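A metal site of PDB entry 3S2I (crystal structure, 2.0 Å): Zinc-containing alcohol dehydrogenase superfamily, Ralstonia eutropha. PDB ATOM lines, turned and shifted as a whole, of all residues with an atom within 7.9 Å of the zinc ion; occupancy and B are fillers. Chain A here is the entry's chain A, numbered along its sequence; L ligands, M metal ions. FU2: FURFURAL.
ND1 of His 63 sits close to OD1 of Asp 43. The side-chain sulfur of Cys 40 lies close to the backbone NH of Thr 42 (3.3 Å). N of Cys 40 lies within hydrogen-bond range of OD2 of Asp 43, at 3.1 Å. The guanidinium group of Arg 333 is in salt-bridge range of the side-chain carboxylate of Glu 64, at 3.2 Å. The backbone NH (N) of Gly 38 lies within hydrogen-bond range of the backbone carbonyl oxygen (O) of Glu 64 (3.1 Å). The side-chain sulfur of Cys 150 lies close to the guanidinium group of Arg 333, 3.6 Å away. The side-chain hydroxyl of Thr 154 lies within hydrogen-bond range of the backbone carbonyl oxygen of Cys 150 (2.7 Å).
Four residues have an atom within 4 Å of the zinc ion: Cys 40, His 63, Glu 64 and Cys 150. The nearest printed residue that does not touch the zinc ion is Arg 333 (4.03 Å).
A ring nitrogen (NE2) of His 63 lies close to an oxygen (OXT) of the ligand (2.4 Å). An oxygen (OXT) of the ligand lies close to the side-chain sulfur (SG) of Cys 40, 3.4 Å away. An oxygen (OXT) of the ligand sits close to the side-chain sulfur (SG) of Cys 150 (2.9 Å). The side-chain hydroxyl of Thr 42 sits at hydrogen-bond distance from an oxygen (O3) of the ligand.
The zinc ion is bound by NE2 of His 63 (2.4 Å), SG of Cys 40 (2.4 Å), OE2 of Glu 64 (2.4 Å) and SG of Cys 150 (2.5 Å). Slightly farther from the zinc ion lies OXT of the ligand (2.7 Å).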
ATOM      1  N   GLY A  38     -21.715 -30.317  22.731  1.00  0.00           N
ATOM      2  CA  GLY A  38     -21.035 -29.618  23.803  1.00  0.00           C
ATOM      3  C   GLY A  38     -20.122 -28.512  23.294  1.00  0.00           C
ATOM      4  O   GLY A  38     -19.581 -28.592  22.191  1.00  0.00           O
ATOM      5  N   VAL A  39     -19.943 -27.490  24.122  1.00  0.00           N
ATOM      6  CA  VAL A  39     -19.076 -26.375  23.779  1.00  0.00           C
ATOM      7  C   VAL A  39     -17.926 -26.261  24.777  1.00  0.00           C
ATOM      8  O   VAL A  39     -18.119 -26.492  25.969  1.00  0.00           O
ATOM      9  CB  VAL A  39     -19.874 -25.049  23.771  1.00  0.00           C
ATOM     10  CG1 VAL A  39     -18.965 -23.887  23.381  1.00  0.00           C
ATOM     11  CG2 VAL A  39     -21.082 -25.150  22.845  1.00  0.00           C
ATOM     12  N   CYS A  40     -16.739 -25.933  24.290  1.00  0.00           N
ATOM     13  CA  CYS A  40     -15.597 -25.729  25.167  1.00  0.00           C
ATOM     14  C   CYS A  40     -14.611 -24.732  24.584  1.00  0.00           C
ATOM     15  O   CYS A  40     -14.739 -24.321  23.423  1.00  0.00           O
ATOM     16  CB  CYS A  40     -14.894 -27.055  25.440  1.00  0.00           C
ATOM     17  SG  CYS A  40     -13.576 -27.405  24.273  1.00  0.00           S
ATOM     18  N   HIS A  41     -13.632 -24.344  25.392  1.00  0.00           N
ATOM     19  CA  HIS A  41     -12.688 -23.279  25.030  1.00  0.00           C
ATOM     20  C   HIS A  41     -11.940 -23.531  23.729  1.00  0.00           C
ATOM     21  O   HIS A  41     -11.479 -22.595  23.079  1.00  0.00           O
ATOM     22  CB  HIS A  41     -11.707 -23.009  26.175  1.00  0.00           C
ATOM     23  CG  HIS A  41     -12.305 -22.266  27.324  1.00  0.00           C
ATOM     24  ND1 HIS A  41     -12.428 -20.889  27.338  1.00  0.00           N
ATOM     25  CD2 HIS A  41     -12.819 -22.700  28.495  1.00  0.00           C
ATOM     26  CE1 HIS A  41     -12.994 -20.517  28.470  1.00  0.00           C
ATOM     27  NE2 HIS A  41     -13.240 -21.599  29.186  1.00  0.00           N
ATOM     28  N   THR A  42     -11.820 -24.807  23.352  1.00  0.00           N
ATOM     29  CA  THR A  42     -11.186 -25.159  22.086  1.00  0.00           C
ATOM     30  C   THR A  42     -11.935 -24.549  20.910  1.00  0.00           C
ATOM     31  O   THR A  42     -11.329 -24.163  19.907  1.00  0.00           O
ATOM     32  CB  THR A  42     -11.083 -26.679  21.906  1.00  0.00           C
ATOM     33  OG1 THR A  42     -10.145 -27.208  22.852  1.00  0.00           O
ATOM     34  CG2 THR A  42     -10.633 -27.035  20.492  1.00  0.00           C
ATOM     35  N   ASP A  43     -13.249 -24.454  21.047  1.00  0.00           N
ATOM     36  CA  ASP A  43     -14.097 -23.872  20.009  1.00  0.00           C
ATOM     37  C   ASP A  43     -13.808 -22.373  19.856  1.00  0.00           C
ATOM     38  O   ASP A  43     -13.927 -21.829  18.760  1.00  0.00           O
ATOM     39  CB  ASP A  43     -15.573 -24.095  20.319  1.00  0.00           C
ATOM     40  CG  ASP A  43     -15.932 -25.568  20.404  1.00  0.00           C
ATOM     41  OD1 ASP A  43     -15.338 -26.372  19.649  1.00  0.00           O
ATOM     42  OD2 ASP A  43     -16.802 -25.935  21.224  1.00  0.00           O
ATOM     43  N   GLY A  62     -17.273 -27.657  16.680  1.00  0.00           N
ATOM     44  CA  GLY A  62     -17.985 -28.676  17.437  1.00  0.00           C
ATOM     45  C   GLY A  62     -17.373 -30.069  17.368  1.00  0.00           C
ATOM     46  O   GLY A  62     -17.541 -30.783  16.386  1.00  0.00           O
ATOM     47  N   HIS A  63     -16.675 -30.448  18.435  1.00  0.00           N
ATOM     48  CA  HIS A  63     -16.087 -31.782  18.527  1.00  0.00           C
ATOM     49  C   HIS A  63     -16.686 -32.522  19.708  1.00  0.00           C
ATOM     50  O   HIS A  63     -16.065 -33.426  20.266  1.00  0.00           O
ATOM     51  CB  HIS A  63     -14.576 -31.684  18.680  1.00  0.00           C
ATOM     52  CG  HIS A  63     -14.154 -30.709  19.732  1.00  0.00           C
ATOM     53  ND1 HIS A  63     -14.074 -29.362  19.497  1.00  0.00           N
ATOM     54  CD2 HIS A  63     -13.831 -30.887  21.036  1.00  0.00           C
ATOM     55  CE1 HIS A  63     -13.698 -28.745  20.604  1.00  0.00           C
ATOM     56  NE2 HIS A  63     -13.549 -29.647  21.555  1.00  0.00           N
ATOM     57  N   GLU A  64     -17.889 -32.124  20.106  1.00  0.00           N
ATOM     58  CA  GLU A  64     -18.595 -32.768  21.211  1.00  0.00           C
ATOM     59  C   GLU A  64     -20.023 -33.103  20.800  1.00  0.00           C
ATOM     60  O   GLU A  64     -20.926 -33.149  21.642  1.00  0.00           O
ATOM     61  CB  GLU A  64     -18.612 -31.857  22.444  1.00  0.00           C
ATOM     62  CG  GLU A  64     -17.241 -31.527  23.004  1.00  0.00           C
ATOM     63  CD  GLU A  64     -17.333 -30.760  24.304  1.00  0.00           C
ATOM     64  OE1 GLU A  64     -18.230 -31.056  25.114  1.00  0.00           O
ATOM     65  OE2 GLU A  64     -16.503 -29.854  24.515  1.00  0.00           O
ATOM     66  N   TRP A  89     -13.029 -35.052  19.015  1.00  0.00           N
ATOM     67  CA  TRP A  89     -11.905 -34.307  18.449  1.00  0.00           C
ATOM     68  C   TRP A  89     -11.137 -35.103  17.393  1.00  0.00           C
ATOM     69  O   TRP A  89     -10.806 -34.578  16.327  1.00  0.00           O
ATOM     70  CB  TRP A  89     -10.966 -33.883  19.582  1.00  0.00           C
ATOM     71  CG  TRP A  89      -9.728 -33.134  19.146  1.00  0.00           C
ATOM     72  CD1 TRP A  89      -8.447 -33.589  19.201  1.00  0.00           C
ATOM     73  CD2 TRP A  89      -9.677 -31.814  18.606  1.00  0.00           C
ATOM     74  NE1 TRP A  89      -7.590 -32.618  18.724  1.00  0.00           N
ATOM     75  CE2 TRP A  89      -8.317 -31.521  18.343  1.00  0.00           C
ATOM     76  CE3 TRP A  89     -10.638 -30.839  18.312  1.00  0.00           C
ATOM     77  CZ2 TRP A  89      -7.901 -30.308  17.810  1.00  0.00           C
ATOM     78  CZ3 TRP A  89     -10.222 -29.629  17.770  1.00  0.00           C
ATOM     79  CH2 TRP A  89      -8.863 -29.368  17.537  1.00  0.00           C
ATOM     80  N   TYR A 122     -21.670 -28.307  15.432  1.00  0.00           N
ATOM     81  CA  TYR A 122     -22.520 -27.127  15.595  1.00  0.00           C
ATOM     82  C   TYR A 122     -23.555 -27.065  14.468  1.00  0.00           C
ATOM     83  O   TYR A 122     -23.837 -26.004  13.924  1.00  0.00           O
ATOM     84  CB  TYR A 122     -21.697 -25.834  15.598  1.00  0.00           C
ATOM     85  CG  TYR A 122     -20.990 -25.520  16.887  1.00  0.00           C
ATOM     86  CD1 TYR A 122     -20.541 -24.227  17.154  1.00  0.00           C
ATOM     87  CD2 TYR A 122     -20.744 -26.498  17.846  1.00  0.00           C
ATOM     88  CE1 TYR A 122     -19.877 -23.917  18.321  1.00  0.00           C
ATOM     89  CE2 TYR A 122     -20.081 -26.195  19.025  1.00  0.00           C
ATOM     90  CZ  TYR A 122     -19.652 -24.899  19.261  1.00  0.00           C
ATOM     91  OH  TYR A 122     -18.988 -24.580  20.425  1.00  0.00           O
ATOM     92  N   ALA A 146     -22.417 -35.410  26.356  1.00  0.00           N
ATOM     93  CA  ALA A 146     -21.633 -34.660  25.373  1.00  0.00           C
ATOM     94  C   ALA A 146     -20.239 -34.257  25.869  1.00  0.00           C
ATOM     95  O   ALA A 146     -19.255 -34.476  25.166  1.00  0.00           O
ATOM     96  CB  ALA A 146     -22.416 -33.437  24.883  1.00  0.00           C
ATOM     97  N   PRO A 147     -20.153 -33.679  27.082  1.00  0.00           N
ATOM     98  CA  PRO A 147     -18.857 -33.217  27.585  1.00  0.00           C
ATOM     99  C   PRO A 147     -17.844 -34.335  27.794  1.00  0.00           C
ATOM    100  O   PRO A 147     -16.640 -34.080  27.799  1.00  0.00           O
ATOM    101  CB  PRO A 147     -19.205 -32.581  28.933  1.00  0.00           C
ATOM    102  CG  PRO A 147     -20.652 -32.205  28.804  1.00  0.00           C
ATOM    103  CD  PRO A 147     -21.264 -33.276  27.965  1.00  0.00           C
ATOM    104  N   LEU A 149     -16.994 -36.499  25.837  1.00  0.00           N
ATOM    105  CA  LEU A 149     -16.249 -36.651  24.590  1.00  0.00           C
ATOM    106  C   LEU A 149     -14.978 -35.806  24.553  1.00  0.00           C
ATOM    107  O   LEU A 149     -14.048 -36.100  23.801  1.00  0.00           O
ATOM    108  CB  LEU A 149     -17.112 -36.288  23.378  1.00  0.00           C
ATOM    109  CG  LEU A 149     -18.444 -37.024  23.177  1.00  0.00           C
ATOM    110  CD1 LEU A 149     -19.036 -36.613  21.846  1.00  0.00           C
ATOM    111  CD2 LEU A 149     -18.245 -38.521  23.227  1.00  0.00           C
ATOM    112  N   CYS A 150     -14.947 -34.744  25.353  1.00  0.00           N
ATOM    113  CA  CYS A 150     -13.801 -33.841  25.386  1.00  0.00           C
ATOM    114  C   CYS A 150     -13.220 -33.690  26.781  1.00  0.00           C
ATOM    115  O   CYS A 150     -12.093 -34.099  27.037  1.00  0.00           O
ATOM    116  CB  CYS A 150     -14.188 -32.462  24.846  1.00  0.00           C
ATOM    117  SG  CYS A 150     -12.995 -31.191  25.280  1.00  0.00           S
ATOM    118  N   ALA A 151     -14.001 -33.085  27.685  1.00  0.00           N
ATOM    119  CA  ALA A 151     -13.559 -32.891  29.062  1.00  0.00           C
ATOM    120  C   ALA A 151     -13.326 -34.221  29.750  1.00  0.00           C
ATOM    121  O   ALA A 151     -12.308 -34.416  30.427  1.00  0.00           O
ATOM    122  CB  ALA A 151     -14.582 -32.055  29.834  1.00  0.00           C
ATOM    123  N   THR A 154     -10.270 -36.401  28.360  1.00  0.00           N
ATOM    124  CA  THR A 154      -9.054 -35.627  28.638  1.00  0.00           C
ATOM    125  C   THR A 154      -8.530 -35.828  30.066  1.00  0.00           C
ATOM    126  O   THR A 154      -7.371 -36.202  30.268  1.00  0.00           O
ATOM    127  CB  THR A 154      -9.258 -34.129  28.379  1.00  0.00           C
ATOM    128  OG1 THR A 154      -9.360 -33.898  26.967  1.00  0.00           O
ATOM    129  CG2 THR A 154      -8.094 -33.321  28.940  1.00  0.00           C
ATOM    130  N   LEU A 178     -13.025 -28.695  33.297  1.00  0.00           N
ATOM    131  CA  LEU A 178     -12.346 -29.990  33.322  1.00  0.00           C
ATOM    132  C   LEU A 178     -12.260 -30.543  34.735  1.00  0.00           C
ATOM    133  O   LEU A 178     -12.640 -31.686  34.984  1.00  0.00           O
ATOM    134  CB  LEU A 178     -10.921 -29.849  32.767  1.00  0.00           C
ATOM    135  CG  LEU A 178     -10.761 -29.558  31.276  1.00  0.00           C
ATOM    136  CD1 LEU A 178      -9.296 -29.706  30.878  1.00  0.00           C
ATOM    137  CD2 LEU A 178     -11.617 -30.492  30.479  1.00  0.00           C
ATOM    138  N   VAL A 288      -7.184 -34.846  25.246  1.00  0.00           N
ATOM    139  CA  VAL A 288      -8.059 -35.908  24.717  1.00  0.00           C
ATOM    140  C   VAL A 288      -7.567 -37.308  25.061  1.00  0.00           C
ATOM    141  O   VAL A 288      -6.982 -37.520  26.114  1.00  0.00           O
ATOM    142  CB  VAL A 288      -8.358 -35.765  23.193  1.00  0.00           C
ATOM    143  CG1 VAL A 288      -9.299 -34.599  22.946  1.00  0.00           C
ATOM    144  CG2 VAL A 288      -7.079 -35.633  22.375  1.00  0.00           C
ATOM    145  N   ARG A 333     -20.132 -27.208  32.082  1.00  0.00           N
ATOM    146  CA  ARG A 333     -20.027 -27.214  30.640  1.00  0.00           C
ATOM    147  C   ARG A 333     -21.333 -26.787  29.999  1.00  0.00           C
ATOM    148  O   ARG A 333     -22.410 -27.133  30.476  1.00  0.00           O
ATOM    149  CB  ARG A 333     -19.646 -28.613  30.132  1.00  0.00           C
ATOM    150  CG  ARG A 333     -18.147 -28.893  30.137  1.00  0.00           C
ATOM    151  CD  ARG A 333     -17.430 -27.910  29.224  1.00  0.00           C
ATOM    152  NE  ARG A 333     -16.006 -28.220  29.084  1.00  0.00           N
ATOM    153  CZ  ARG A 333     -15.516 -29.021  28.145  1.00  0.00           C
ATOM    154  NH1 ARG A 333     -14.207 -29.249  28.089  1.00  0.00           N
ATOM    155  NH2 ARG A 333     -16.316 -29.603  27.273  1.00  0.00           N
HETATM  156  C1  FU2 L   1     -10.755 -30.920  22.891  1.00  0.00           C
HETATM  157  C2  FU2 L   1      -9.483 -30.587  22.191  1.00  0.00           C
HETATM  158  O3  FU2 L   1      -9.236 -29.476  21.466  1.00  0.00           O
HETATM  159  C4  FU2 L   1      -7.985 -29.465  20.977  1.00  0.00           C
HETATM  160  C5  FU2 L   1      -7.371 -30.637  21.405  1.00  0.00           C
HETATM  161  C6  FU2 L   1      -8.308 -31.331  22.169  1.00  0.00           C
HETATM  162  OXT FU2 L   1     -11.694 -29.920  23.068  1.00  0.00           O
HETATM  163 ZN    ZN M   1     -14.246 -29.635  23.811  1.00  0.00          ZN
